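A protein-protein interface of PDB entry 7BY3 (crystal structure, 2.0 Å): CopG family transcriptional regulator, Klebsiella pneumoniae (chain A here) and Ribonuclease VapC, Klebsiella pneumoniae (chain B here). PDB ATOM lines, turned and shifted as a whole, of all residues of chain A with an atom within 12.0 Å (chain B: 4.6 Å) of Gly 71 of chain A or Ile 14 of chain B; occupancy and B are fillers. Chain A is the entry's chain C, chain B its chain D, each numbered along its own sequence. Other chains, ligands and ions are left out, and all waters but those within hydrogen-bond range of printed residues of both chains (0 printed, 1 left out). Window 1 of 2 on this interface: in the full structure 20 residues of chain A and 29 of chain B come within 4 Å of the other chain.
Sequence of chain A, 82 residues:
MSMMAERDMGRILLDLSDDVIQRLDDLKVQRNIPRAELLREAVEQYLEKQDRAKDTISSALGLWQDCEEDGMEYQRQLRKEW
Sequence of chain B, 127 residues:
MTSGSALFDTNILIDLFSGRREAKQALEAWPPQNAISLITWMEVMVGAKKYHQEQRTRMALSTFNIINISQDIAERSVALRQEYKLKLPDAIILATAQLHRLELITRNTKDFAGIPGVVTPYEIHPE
N of Leu 63 of chain A lies within hydrogen-bond range of O of Phe 17 of chain B. The backbone NH of Trp 64 of chain A is in hydrogen-bond range of the backbone carbonyl oxygen of Phe 17 of chain B, at 2.8 Å. The side-chain hydroxyl (OG) of Ser 18 of chain B lies within hydrogen-bond range of the side-chain sulfur (SG) of Cys 67 of chain A (3.0 Å). The side-chain carboxylate (OD1) of Asp 70 of chain A is in salt-bridge range of the guanidinium group (NH2) of Arg 20 of chain B, at 3.5 Å. OD1 of Asp 70 of chain A is in salt-bridge range of NH2 of Arg 107 of chain B (3.3 Å). N of Gly 71 of chain A lies within hydrogen-bond range of OD1 of Asp 15 of chain B, at 2.7 Å. The side-chain sulfur (SD) of Met 72 of chain A lies close to the side-chain amide nitrogen (ND2) of Asn 11 of chain B (3.8 Å). The backbone NH (N) of Thr 10 of chain B sits close to the side-chain amide oxygen (OE1) of Gln 75 of chain A, 3.5 Å away. The backbone NH of Asn 11 of chain B lies within hydrogen-bond range of the side-chain amide oxygen of Gln 75 of chain A, at 3.1 Å. O of Ala 60 of chain A lies close to O of Leu 16 of chain B, 3.3 Å away.
NE2 of Gln 75 of chain A sits close to NH2 of Arg 79 of chain A, at 2.8 Å. OG of Ser 18 of chain B lies within hydrogen-bond range of O of Ile 14 of chain B (2.6 Å). OD1 of Asp 15 of chain B lies within salt-bridge range of NH1 of Arg 20 of chain B (3.6 Å).
Among the printed residues, merely in contact across the chains: Leu 61 of chain A with Arg 20 of chain B (3.2 Å), Ala 60 of chain A with Phe 17 of chain B (3.3 Å), Gly 62 of chain A with Phe 17 of chain B (3.3 Å), Met 72 of chain A with Arg 107 of chain B (3.4 Å), Trp 64 of chain A with Val 44 of chain B (3.5 Å), Leu 61 of chain A with Leu 16 of chain B (3.6 Å), Trp 64 of chain A with Ile 14 of chain B (3.6 Å), Gly 62 of chain A with Leu 16 of chain B (3.6 Å), Gly 71 of chain A with Asn 11 of chain B (3.6 Å), Tyr 74 of chain A with Ile 14 of chain B (3.6 Å), Gly 71 of chain A with Ile 14 of chain B (3.6 Å), Glu 69 of chain A with Ser 18 of chain B (3.6 Å), Ile 57 of chain A with Leu 16 of chain B (3.8 Å), Asp 70 of chain A with Asp 15 of chain B (3.9 Å) and Trp 64 of chain A with Ser 18 of chain B (3.99 Å).
Of the printed residues of chain B, Tyr 74 of chain A touches Ile 14. Ile 12 of chain B touches none of the printed residues of chain A. Asp 15 of chain B touches just these residues of chain A: Asp 70 (3.9 Å) and Gly 71 (2.7 Å). Phe 17 of chain B touches just these residues of chain A: Ala 60, Gly 62, Leu 63 and Trp 64. Of the printed residues of chain A, Ser 18 of chain B touches Trp 64, Cys 67 and Glu 69. Arg 20 of chain B touches just these residues of chain A: Leu 61 (3.2 Å) and Asp 70 (2.4 Å). The nearest residue of chain B that does not touch Gly 71 of chain A is Arg 107 of chain B (4.1 Å).
Of the 24 printed residues of chain A, 13 touch a printed residue of chain B. Hydrophobic or aromatic side chains of chain A within 4 Å of the printed part of chain B: Ile 57, Ala 60, Leu 61, Leu 63, Trp 64, Met 72 and Tyr 74. Printed residues of chain B that touch a printed residue of chain A: Thr 10, Asn 11, Ile 14, Asp 15, Leu 16, Phe 17, Ser 18, Arg 20, Val 44 and Arg 107.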
ATOM      1  N   ILE A  57     -31.588 -10.458  38.253  1.00  0.00           N
ATOM      2  CA  ILE A  57     -31.118 -11.432  37.276  1.00  0.00           C
ATOM      3  C   ILE A  57     -32.171 -11.704  36.201  1.00  0.00           C
ATOM      4  O   ILE A  57     -31.842 -11.917  35.034  1.00  0.00           O
ATOM      5  CB  ILE A  57     -30.720 -12.748  37.974  1.00  0.00           C
ATOM      6  CG1 ILE A  57     -29.547 -12.498  38.922  1.00  0.00           C
ATOM      7  CG2 ILE A  57     -30.355 -13.821  36.960  1.00  0.00           C
ATOM      8  CD1 ILE A  57     -29.086 -13.727  39.662  1.00  0.00           C
ATOM      9  N   SER A  59     -34.512  -9.621  35.014  1.00  0.00           N
ATOM     10  CA  SER A  59     -34.652  -8.502  34.087  1.00  0.00           C
ATOM     11  C   SER A  59     -33.422  -8.372  33.194  1.00  0.00           C
ATOM     12  O   SER A  59     -33.477  -7.754  32.133  1.00  0.00           O
ATOM     13  CB  SER A  59     -34.894  -7.198  34.847  1.00  0.00           C
ATOM     14  OG  SER A  59     -36.206  -7.157  35.378  1.00  0.00           O
ATOM     15  N   ALA A  60     -32.315  -8.963  33.629  1.00  0.00           N
ATOM     16  CA  ALA A  60     -31.095  -8.960  32.837  1.00  0.00           C
ATOM     17  C   ALA A  60     -31.172 -10.011  31.737  1.00  0.00           C
ATOM     18  O   ALA A  60     -30.390  -9.989  30.788  1.00  0.00           O
ATOM     19  CB  ALA A  60     -29.888  -9.209  33.722  1.00  0.00           C
ATOM     20  N   LEU A  61     -32.130 -10.923  31.868  1.00  0.00           N
ATOM     21  CA  LEU A  61     -32.243 -12.063  30.966  1.00  0.00           C
ATOM     22  C   LEU A  61     -33.393 -11.999  29.964  1.00  0.00           C
ATOM     23  O   LEU A  61     -34.558 -11.900  30.346  1.00  0.00           O
ATOM     24  CB  LEU A  61     -32.394 -13.351  31.780  1.00  0.00           C
ATOM     25  CG  LEU A  61     -32.659 -14.617  30.956  1.00  0.00           C
ATOM     26  CD1 LEU A  61     -31.406 -15.460  30.811  1.00  0.00           C
ATOM     27  CD2 LEU A  61     -33.798 -15.431  31.555  1.00  0.00           C
ATOM     28  N   GLY A  62     -33.055 -12.029  28.677  1.00  0.00           N
ATOM     29  CA  GLY A  62     -31.813 -11.460  28.189  1.00  0.00           C
ATOM     30  C   GLY A  62     -32.050  -9.973  28.030  1.00  0.00           C
ATOM     31  O   GLY A  62     -33.051  -9.586  27.430  1.00  0.00           O
ATOM     32  N   LEU A  63     -31.151  -9.133  28.524  1.00  0.00           N
ATOM     33  CA  LEU A  63     -31.376  -7.699  28.399  1.00  0.00           C
ATOM     34  C   LEU A  63     -30.961  -7.197  27.027  1.00  0.00           C
ATOM     35  O   LEU A  63     -31.519  -6.224  26.518  1.00  0.00           O
ATOM     36  CB  LEU A  63     -30.641  -6.923  29.489  1.00  0.00           C
ATOM     37  CG  LEU A  63     -30.826  -5.405  29.416  1.00  0.00           C
ATOM     38  CD1 LEU A  63     -32.286  -5.026  29.629  1.00  0.00           C
ATOM     39  CD2 LEU A  63     -29.941  -4.715  30.432  1.00  0.00           C
ATOM     40  N   TRP A  64     -30.017  -7.877  26.391  1.00  0.00           N
ATOM     41  CA  TRP A  64     -29.547  -7.362  25.126  1.00  0.00           C
ATOM     42  C   TRP A  64     -30.450  -7.943  24.055  1.00  0.00           C
ATOM     43  O   TRP A  64     -30.363  -9.120  23.706  1.00  0.00           O
ATOM     44  CB  TRP A  64     -28.079  -7.730  24.884  1.00  0.00           C
ATOM     45  CG  TRP A  64     -27.109  -7.158  25.893  1.00  0.00           C
ATOM     46  CD1 TRP A  64     -27.363  -6.192  26.824  1.00  0.00           C
ATOM     47  CD2 TRP A  64     -25.732  -7.525  26.069  1.00  0.00           C
ATOM     48  NE1 TRP A  64     -26.234  -5.935  27.563  1.00  0.00           N
ATOM     49  CE2 TRP A  64     -25.220  -6.742  27.118  1.00  0.00           C
ATOM     50  CE3 TRP A  64     -24.887  -8.444  25.435  1.00  0.00           C
ATOM     51  CZ2 TRP A  64     -23.899  -6.845  27.552  1.00  0.00           C
ATOM     52  CZ3 TRP A  64     -23.576  -8.544  25.869  1.00  0.00           C
ATOM     53  CH2 TRP A  64     -23.095  -7.750  26.916  1.00  0.00           C
ATOM     54  N   GLN A  65     -31.302  -7.073  23.526  1.00  0.00           N
ATOM     55  CA  GLN A  65     -32.289  -7.435  22.525  1.00  0.00           C
ATOM     56  C   GLN A  65     -31.646  -7.148  21.182  1.00  0.00           C
ATOM     57  O   GLN A  65     -31.439  -5.978  20.864  1.00  0.00           O
ATOM     58  CB  GLN A  65     -33.580  -6.629  22.742  1.00  0.00           C
ATOM     59  CG  GLN A  65     -34.278  -6.100  21.498  1.00  0.00           C
ATOM     60  CD  GLN A  65     -35.279  -5.010  21.822  1.00  0.00           C
ATOM     61  OE1 GLN A  65     -35.375  -4.565  22.964  1.00  0.00           O
ATOM     62  NE2 GLN A  65     -36.001  -4.546  20.809  1.00  0.00           N
ATOM     63  N   ASP A  66     -31.449  -8.218  20.394  1.00  0.00           N
ATOM     64  CA  ASP A  66     -30.515  -8.389  19.242  1.00  0.00           C
ATOM     65  C   ASP A  66     -29.110  -8.992  19.514  1.00  0.00           C
ATOM     66  O   ASP A  66     -28.319  -9.101  18.576  1.00  0.00           O
ATOM     67  CB  ASP A  66     -30.313  -7.078  18.443  1.00  0.00           C
ATOM     68  CG  ASP A  66     -29.436  -6.051  19.157  1.00  0.00           C
ATOM     69  OD1 ASP A  66     -28.941  -6.328  20.264  1.00  0.00           O
ATOM     70  OD2 ASP A  66     -29.277  -4.936  18.619  1.00  0.00           O
ATOM     71  N   CYS A  67     -28.770  -9.368  20.748  1.00  0.00           N
ATOM     72  CA  CYS A  67     -27.493 -10.075  20.960  1.00  0.00           C
ATOM     73  C   CYS A  67     -27.607 -11.606  20.893  1.00  0.00           C
ATOM     74  O   CYS A  67     -28.184 -12.237  21.777  1.00  0.00           O
ATOM     75  CB  CYS A  67     -26.876  -9.693  22.304  1.00  0.00           C
ATOM     76  SG  CYS A  67     -25.353 -10.604  22.697  1.00  0.00           S
ATOM     77  N   GLU A  68     -27.045 -12.186  19.834  1.00  0.00           N
ATOM     78  CA  GLU A  68     -27.004 -13.640  19.650  1.00  0.00           C
ATOM     79  C   GLU A  68     -25.668 -14.296  20.017  1.00  0.00           C
ATOM     80  O   GLU A  68     -25.506 -15.507  19.861  1.00  0.00           O
ATOM     81  CB  GLU A  68     -27.354 -13.991  18.201  1.00  0.00           C
ATOM     82  CG  GLU A  68     -28.845 -14.162  17.931  1.00  0.00           C
ATOM     83  CD  GLU A  68     -29.580 -12.850  17.709  1.00  0.00           C
ATOM     84  OE1 GLU A  68     -30.411 -12.793  16.779  1.00  0.00           O
ATOM     85  OE2 GLU A  68     -29.342 -11.884  18.461  1.00  0.00           O
ATOM     86  N   GLU A  69     -24.714 -13.497  20.487  1.00  0.00           N
ATOM     87  CA  GLU A  69     -23.347 -13.969  20.704  1.00  0.00           C
ATOM     88  C   GLU A  69     -23.222 -14.967  21.851  1.00  0.00           C
ATOM     89  O   GLU A  69     -23.947 -14.884  22.843  1.00  0.00           O
ATOM     90  CB  GLU A  69     -22.426 -12.787  20.951  1.00  0.00           C
ATOM     91  N   ASP A  70     -22.293 -15.907  21.708  1.00  0.00           N
ATOM     92  CA  ASP A  70     -21.954 -16.825  22.789  1.00  0.00           C
ATOM     93  C   ASP A  70     -20.934 -16.166  23.712  1.00  0.00           C
ATOM     94  O   ASP A  70     -19.904 -15.671  23.254  1.00  0.00           O
ATOM     95  CB  ASP A  70     -21.404 -18.142  22.238  1.00  0.00           C
ATOM     96  CG  ASP A  70     -21.281 -19.214  23.304  1.00  0.00           C
ATOM     97  OD1 ASP A  70     -22.287 -19.493  23.987  1.00  0.00           O
ATOM     98  OD2 ASP A  70     -20.176 -19.772  23.463  1.00  0.00           O
ATOM     99  N   GLY A  71     -21.227 -16.168  25.009  1.00  0.00           N
ATOM    100  CA  GLY A  71     -20.416 -15.471  25.992  1.00  0.00           C
ATOM    101  C   GLY A  71     -18.945 -15.839  25.991  1.00  0.00           C
ATOM    102  O   GLY A  71     -18.083 -14.970  26.134  1.00  0.00           O
ATOM    103  N   MET A  72     -18.658 -17.126  25.832  1.00  0.00           N
ATOM    104  CA  MET A  72     -17.279 -17.598  25.794  1.00  0.00           C
ATOM    105  C   MET A  72     -16.568 -17.144  24.523  1.00  0.00           C
ATOM    106  O   MET A  72     -15.381 -16.819  24.550  1.00  0.00           O
ATOM    107  CB  MET A  72     -17.232 -19.121  25.906  1.00  0.00           C
ATOM    108  CG  MET A  72     -17.146 -19.620  27.329  1.00  0.00           C
ATOM    109  SD  MET A  72     -15.681 -19.029  28.199  1.00  0.00           S
ATOM    110  CE  MET A  72     -14.379 -19.737  27.198  1.00  0.00           C
ATOM    111  N   GLU A  73     -17.298 -17.133  23.411  1.00  0.00           N
ATOM    112  CA  GLU A  73     -16.763 -16.650  22.142  1.00  0.00           C
ATOM    113  C   GLU A  73     -16.495 -15.156  22.233  1.00  0.00           C
ATOM    114  O   GLU A  73     -15.437 -14.674  21.826  1.00  0.00           O
ATOM    115  CB  GLU A  73     -17.736 -16.931  20.999  1.00  0.00           C
ATOM    116  CG  GLU A  73     -18.049 -18.395  20.779  1.00  0.00           C
ATOM    117  CD  GLU A  73     -19.122 -18.593  19.730  1.00  0.00           C
ATOM    118  OE1 GLU A  73     -19.729 -17.585  19.311  1.00  0.00           O
ATOM    119  OE2 GLU A  73     -19.364 -19.750  19.331  1.00  0.00           O
ATOM    120  N   TYR A  74     -17.483 -14.444  22.765  1.00  0.00           N
ATOM    121  CA  TYR A  74     -17.384 -13.025  23.076  1.00  0.00           C
ATOM    122  C   TYR A  74     -16.083 -12.758  23.816  1.00  0.00           C
ATOM    123  O   TYR A  74     -15.242 -11.980  23.361  1.00  0.00           O
ATOM    124  CB  TYR A  74     -18.591 -12.586  23.914  1.00  0.00           C
ATOM    125  CG  TYR A  74     -18.634 -11.116  24.274  1.00  0.00           C
ATOM    126  CD1 TYR A  74     -17.835 -10.603  25.288  1.00  0.00           C
ATOM    127  CD2 TYR A  74     -19.498 -10.247  23.616  1.00  0.00           C
ATOM    128  CE1 TYR A  74     -17.876  -9.268  25.623  1.00  0.00           C
ATOM    129  CE2 TYR A  74     -19.548  -8.907  23.948  1.00  0.00           C
ATOM    130  CZ  TYR A  74     -18.734  -8.423  24.952  1.00  0.00           C
ATOM    131  OH  TYR A  74     -18.773  -7.093  25.292  1.00  0.00           O
ATOM    132  N   GLN A  75     -15.948 -13.403  24.969  1.00  0.00           N
ATOM    133  CA  GLN A  75     -14.773 -13.284  25.822  1.00  0.00           C
ATOM    134  C   GLN A  75     -13.446 -13.467  25.089  1.00  0.00           C
ATOM    135  O   GLN A  75     -12.549 -12.635  25.211  1.00  0.00           O
ATOM    136  CB  GLN A  75     -14.859 -14.303  26.957  1.00  0.00           C
ATOM    137  CG  GLN A  75     -13.742 -14.162  27.955  1.00  0.00           C
ATOM    138  CD  GLN A  75     -14.161 -13.335  29.141  1.00  0.00           C
ATOM    139  OE1 GLN A  75     -14.793 -13.835  30.072  1.00  0.00           O
ATOM    140  NE2 GLN A  75     -13.856 -12.043  29.091  1.00  0.00           N
ATOM    141  N   ARG A  76     -13.330 -14.555  24.331  1.00  0.00           N
ATOM    142  CA  ARG A  76     -12.088 -14.878  23.631  1.00  0.00           C
ATOM    143  C   ARG A  76     -11.678 -13.743  22.701  1.00  0.00           C
ATOM    144  O   ARG A  76     -10.491 -13.485  22.500  1.00  0.00           O
ATOM    145  CB  ARG A  76     -12.235 -16.179  22.836  1.00  0.00           C
ATOM    146  CG  ARG A  76     -10.916 -16.729  22.319  1.00  0.00           C
ATOM    147  CD  ARG A  76     -10.072 -17.248  23.471  1.00  0.00           C
ATOM    148  NE  ARG A  76      -8.646 -17.001  23.274  1.00  0.00           N
ATOM    149  CZ  ARG A  76      -8.022 -15.908  23.699  1.00  0.00           C
ATOM    150  NH1 ARG A  76      -8.703 -14.966  24.333  1.00  0.00           N
ATOM    151  NH2 ARG A  76      -6.723 -15.753  23.487  1.00  0.00           N
ATOM    152  N   GLN A  77     -12.676 -13.063  22.145  1.00  0.00           N
ATOM    153  CA  GLN A  77     -12.436 -11.939  21.252  1.00  0.00           C
ATOM    154  C   GLN A  77     -11.850 -10.733  21.973  1.00  0.00           C
ATOM    155  O   GLN A  77     -10.885 -10.149  21.497  1.00  0.00           O
ATOM    156  CB  GLN A  77     -13.731 -11.532  20.541  1.00  0.00           C
ATOM    157  CG  GLN A  77     -14.013 -12.312  19.267  1.00  0.00           C
ATOM    158  CD  GLN A  77     -12.996 -12.028  18.178  1.00  0.00           C
ATOM    159  OE1 GLN A  77     -11.951 -12.674  18.105  1.00  0.00           O
ATOM    160  NE2 GLN A  77     -13.294 -11.051  17.330  1.00  0.00           N
ATOM    161  N   LEU A  78     -12.425 -10.344  23.107  1.00  0.00           N
ATOM    162  CA  LEU A  78     -11.946  -9.144  23.786  1.00  0.00           C
ATOM    163  C   LEU A  78     -10.683  -9.420  24.603  1.00  0.00           C
ATOM    164  O   LEU A  78      -9.897  -8.510  24.883  1.00  0.00           O
ATOM    165  CB  LEU A  78     -13.026  -8.528  24.673  1.00  0.00           C
ATOM    166  CG  LEU A  78     -12.550  -7.172  25.209  1.00  0.00           C
ATOM    167  CD1 LEU A  78     -13.009  -6.050  24.299  1.00  0.00           C
ATOM    168  CD2 LEU A  78     -12.984  -6.908  26.624  1.00  0.00           C
ATOM    169  N   ARG A  79     -10.463 -10.673  24.975  1.00  0.00           N
ATOM    170  CA  ARG A  79      -9.186 -11.002  25.576  1.00  0.00           C
ATOM    171  C   ARG A  79      -8.112 -10.802  24.503  1.00  0.00           C
ATOM    172  O   ARG A  79      -6.983 -10.426  24.823  1.00  0.00           O
ATOM    173  CB  ARG A  79      -9.191 -12.418  26.156  1.00  0.00           C
ATOM    174  CG  ARG A  79     -10.197 -12.625  27.292  1.00  0.00           C
ATOM    175  CD  ARG A  79      -9.722 -11.997  28.598  1.00  0.00           C
ATOM    176  NE  ARG A  79     -10.828 -11.772  29.527  1.00  0.00           N
ATOM    177  CZ  ARG A  79     -11.138 -12.582  30.535  1.00  0.00           C
ATOM    178  NH1 ARG A  79     -10.427 -13.676  30.752  1.00  0.00           N
ATOM    179  NH2 ARG A  79     -12.162 -12.300  31.324  1.00  0.00           N
ATOM    180  N   LYS A  80      -8.474 -11.051  23.241  1.00  0.00           N
ATOM    181  CA  LYS A  80      -7.663 -10.632  22.089  1.00  0.00           C
ATOM    182  C   LYS A  80      -8.200  -9.310  21.470  1.00  0.00           C
ATOM    183  O   LYS A  80      -7.849  -8.927  20.353  1.00  0.00           O
ATOM    184  CB  LYS A  80      -7.517 -11.765  21.054  1.00  0.00           C
ATOM    185  CG  LYS A  80      -6.446 -11.445  19.992  1.00  0.00           C
ATOM    186  CD  LYS A  80      -5.968 -12.603  19.131  1.00  0.00           C
ATOM    187  CE  LYS A  80      -4.933 -12.078  18.134  1.00  0.00           C
ATOM    188  NZ  LYS A  80      -5.389 -10.776  17.553  1.00  0.00           N
ATOM    189  N   GLU A  81      -9.137  -8.681  22.184  1.00  0.00           N
ATOM    190  CA  GLU A  81      -9.542  -7.237  22.114  1.00  0.00           C
ATOM    191  C   GLU A  81     -10.190  -6.676  20.830  1.00  0.00           C
ATOM    192  O   GLU A  81     -10.469  -5.477  20.791  1.00  0.00           O
ATOM    193  CB  GLU A  81      -8.383  -6.291  22.542  1.00  0.00           C
ATOM    194  CG  GLU A  81      -6.960  -6.759  22.288  1.00  0.00           C
ATOM    195  CD  GLU A  81      -6.034  -6.523  23.450  1.00  0.00           C
ATOM    196  OE1 GLU A  81      -5.886  -7.466  24.250  1.00  0.00           O
ATOM    197  OE2 GLU A  81      -5.398  -5.462  23.529  1.00  0.00           O
ATOM    198  N   THR B  10     -16.520 -12.805  32.925  1.00  0.00           N
ATOM    199  CA  THR B  10     -17.304 -12.069  31.937  1.00  0.00           C
ATOM    200  C   THR B  10     -18.251 -12.958  31.129  1.00  0.00           C
ATOM    201  O   THR B  10     -19.405 -12.593  30.904  1.00  0.00           O
ATOM    202  CB  THR B  10     -16.374 -11.312  30.969  1.00  0.00           C
ATOM    203  OG1 THR B  10     -15.672 -10.283  31.676  1.00  0.00           O
ATOM    204  CG2 THR B  10     -17.149 -10.683  29.830  1.00  0.00           C
ATOM    205  N   ASN B  11     -17.763 -14.124  30.712  1.00  0.00           N
ATOM    206  CA  ASN B  11     -18.511 -15.014  29.821  1.00  0.00           C
ATOM    207  C   ASN B  11     -19.897 -15.390  30.347  1.00  0.00           C
ATOM    208  O   ASN B  11     -20.849 -15.513  29.575  1.00  0.00           O
ATOM    209  CB  ASN B  11     -17.702 -16.288  29.545  1.00  0.00           C
ATOM    210  CG  ASN B  11     -17.422 -17.095  30.803  1.00  0.00           C
ATOM    211  OD1 ASN B  11     -18.280 -17.837  31.280  1.00  0.00           O
ATOM    212  ND2 ASN B  11     -16.215 -16.963  31.338  1.00  0.00           N
ATOM    213  N   ILE B  12     -20.006 -15.565  31.658  1.00  0.00           N
ATOM    214  CA  ILE B  12     -21.278 -15.916  32.277  1.00  0.00           C
ATOM    215  C   ILE B  12     -22.229 -14.724  32.266  1.00  0.00           C
ATOM    216  O   ILE B  12     -23.425 -14.877  32.025  1.00  0.00           O
ATOM    217  CB  ILE B  12     -21.073 -16.416  33.718  1.00  0.00           C
ATOM    218  CG1 ILE B  12     -20.306 -17.735  33.698  1.00  0.00           C
ATOM    219  CG2 ILE B  12     -22.408 -16.604  34.424  1.00  0.00           C
ATOM    220  CD1 ILE B  12     -19.792 -18.150  35.035  1.00  0.00           C
ATOM    221  N   LEU B  13     -21.691 -13.533  32.508  1.00  0.00           N
ATOM    222  CA  LEU B  13     -22.499 -12.320  32.470  1.00  0.00           C
ATOM    223  C   LEU B  13     -22.961 -12.008  31.047  1.00  0.00           C
ATOM    224  O   LEU B  13     -24.090 -11.567  30.841  1.00  0.00           O
ATOM    225  CB  LEU B  13     -21.726 -11.136  33.055  1.00  0.00           C
ATOM    226  CG  LEU B  13     -22.084 -10.750  34.494  1.00  0.00           C
ATOM    227  CD1 LEU B  13     -21.154  -9.674  35.012  1.00  0.00           C
ATOM    228  CD2 LEU B  13     -23.525 -10.277  34.574  1.00  0.00           C
ATOM    229  N   ILE B  14     -22.092 -12.248  30.069  1.00  0.00           N
ATOM    230  CA  ILE B  14     -22.453 -12.052  28.668  1.00  0.00           C
ATOM    231  C   ILE B  14     -23.595 -12.981  28.282  1.00  0.00           C
ATOM    232  O   ILE B  14     -24.547 -12.567  27.625  1.00  0.00           O
ATOM    233  CB  ILE B  14     -21.261 -12.297  27.724  1.00  0.00           C
ATOM    234  CG1 ILE B  14     -20.105 -11.365  28.072  1.00  0.00           C
ATOM    235  CG2 ILE B  14     -21.673 -12.082  26.277  1.00  0.00           C
ATOM    236  CD1 ILE B  14     -20.477  -9.903  28.060  1.00  0.00           C
ATOM    237  N   ASP B  15     -23.491 -14.237  28.702  1.00  0.00           N
ATOM    238  CA  ASP B  15     -24.523 -15.232  28.438  1.00  0.00           C
ATOM    239  C   ASP B  15     -25.856 -14.834  29.056  1.00  0.00           C
ATOM    240  O   ASP B  15     -26.914 -15.099  28.490  1.00  0.00           O
ATOM    241  CB  ASP B  15     -24.095 -16.600  28.968  1.00  0.00           C
ATOM    242  CG  ASP B  15     -23.033 -17.252  28.107  1.00  0.00           C
ATOM    243  OD1 ASP B  15     -23.021 -17.001  26.884  1.00  0.00           O
ATOM    244  OD2 ASP B  15     -22.214 -18.019  28.653  1.00  0.00           O
ATOM    245  N   LEU B  16     -25.796 -14.198  30.222  1.00  0.00           N
ATOM    246  CA  LEU B  16     -26.999 -13.756  30.916  1.00  0.00           C
ATOM    247  C   LEU B  16     -27.742 -12.688  30.125  1.00  0.00           C
ATOM    248  O   LEU B  16     -28.935 -12.824  29.853  1.00  0.00           O
ATOM    249  CB  LEU B  16     -26.653 -13.219  32.305  1.00  0.00           C
ATOM    250  CG  LEU B  16     -27.837 -12.640  33.081  1.00  0.00           C
ATOM    251  CD1 LEU B  16     -28.876 -13.716  33.364  1.00  0.00           C
ATOM    252  CD2 LEU B  16     -27.373 -11.977  34.364  1.00  0.00           C
ATOM    253  N   PHE B  17     -27.032 -11.626  29.758  1.00  0.00           N
ATOM    254  CA  PHE B  17     -27.630 -10.538  28.994  1.00  0.00           C
ATOM    255  C   PHE B  17     -28.016 -11.001  27.592  1.00  0.00           C
ATOM    256  O   PHE B  17     -28.886 -10.411  26.953  1.00  0.00           O
ATOM    257  CB  PHE B  17     -26.675  -9.345  28.910  1.00  0.00           C
ATOM    258  CG  PHE B  17     -26.376  -8.711  30.239  1.00  0.00           C
ATOM    259  CD1 PHE B  17     -27.379  -8.096  30.970  1.00  0.00           C
ATOM    260  CD2 PHE B  17     -25.090  -8.717  30.751  1.00  0.00           C
ATOM    261  CE1 PHE B  17     -27.105  -7.509  32.191  1.00  0.00           C
ATOM    262  CE2 PHE B  17     -24.810  -8.134  31.971  1.00  0.00           C
ATOM    263  CZ  PHE B  17     -25.818  -7.528  32.691  1.00  0.00           C
ATOM    264  N   SER B  18     -27.367 -12.064  27.123  1.00  0.00           N
ATOM    265  CA  SER B  18     -27.647 -12.606  25.799  1.00  0.00           C
ATOM    266  C   SER B  18     -28.826 -13.578  25.830  1.00  0.00           C
ATOM    267  O   SER B  18     -29.193 -14.147  24.802  1.00  0.00           O
ATOM    268  CB  SER B  18     -26.410 -13.303  25.229  1.00  0.00           C
ATOM    269  OG  SER B  18     -25.324 -12.399  25.113  1.00  0.00           O
ATOM    270  N   ARG B  20     -29.405 -16.468  28.027  1.00  0.00           N
ATOM    271  CA  ARG B  20     -29.206 -17.880  28.340  1.00  0.00           C
ATOM    272  C   ARG B  20     -29.574 -18.225  29.785  1.00  0.00           C
ATOM    273  O   ARG B  20     -29.035 -17.648  30.727  1.00  0.00           O
ATOM    274  CB  ARG B  20     -27.760 -18.283  28.062  1.00  0.00           C
ATOM    275  CG  ARG B  20     -27.454 -18.457  26.589  1.00  0.00           C
ATOM    276  CD  ARG B  20     -26.212 -19.298  26.395  1.00  0.00           C
ATOM    277  NE  ARG B  20     -26.238 -20.029  25.131  1.00  0.00           N
ATOM    278  CZ  ARG B  20     -25.446 -19.767  24.097  1.00  0.00           C
ATOM    279  NH1 ARG B  20     -24.555 -18.788  24.173  1.00  0.00           N
ATOM    280  NH2 ARG B  20     -25.542 -20.486  22.987  1.00  0.00           N
ATOM    281  N   VAL B  44     -18.156  -6.140  29.766  1.00  0.00           N
ATOM    282  CA  VAL B  44     -19.605  -6.208  29.627  1.00  0.00           C
ATOM    283  C   VAL B  44     -20.188  -4.901  29.085  1.00  0.00           C
ATOM    284  O   VAL B  44     -21.082  -4.915  28.235  1.00  0.00           O
ATOM    285  CB  VAL B  44     -20.272  -6.551  30.978  1.00  0.00           C
ATOM    286  CG1 VAL B  44     -21.786  -6.449  30.875  1.00  0.00           C
ATOM    287  CG2 VAL B  44     -19.862  -7.944  31.429  1.00  0.00           C
ATOM    288  N   ARG B 107     -16.731 -20.286  32.468  1.00  0.00           N
ATOM    289  CA  ARG B 107     -16.921 -21.371  31.516  1.00  0.00           C
ATOM    290  C   ARG B 107     -15.603 -21.780  30.876  1.00  0.00           C
ATOM    291  O   ARG B 107     -15.578 -22.651  30.009  1.00  0.00           O
ATOM    292  CB  ARG B 107     -17.899 -20.975  30.414  1.00  0.00           C
ATOM    293  CG  ARG B 107     -19.346 -20.842  30.817  1.00  0.00           C
ATOM    294  CD  ARG B 107     -20.135 -20.327  29.625  1.00  0.00           C
ATOM    295  NE  ARG B 107     -19.942 -21.164  28.443  1.00  0.00           N
ATOM    296  CZ  ARG B 107     -20.346 -20.837  27.218  1.00  0.00           C
ATOM    297  NH1 ARG B 107     -20.130 -21.661  26.202  1.00  0.00           N
ATOM    298  NH2 ARG B 107     -20.959 -19.681  27.008  1.00  0.00           N
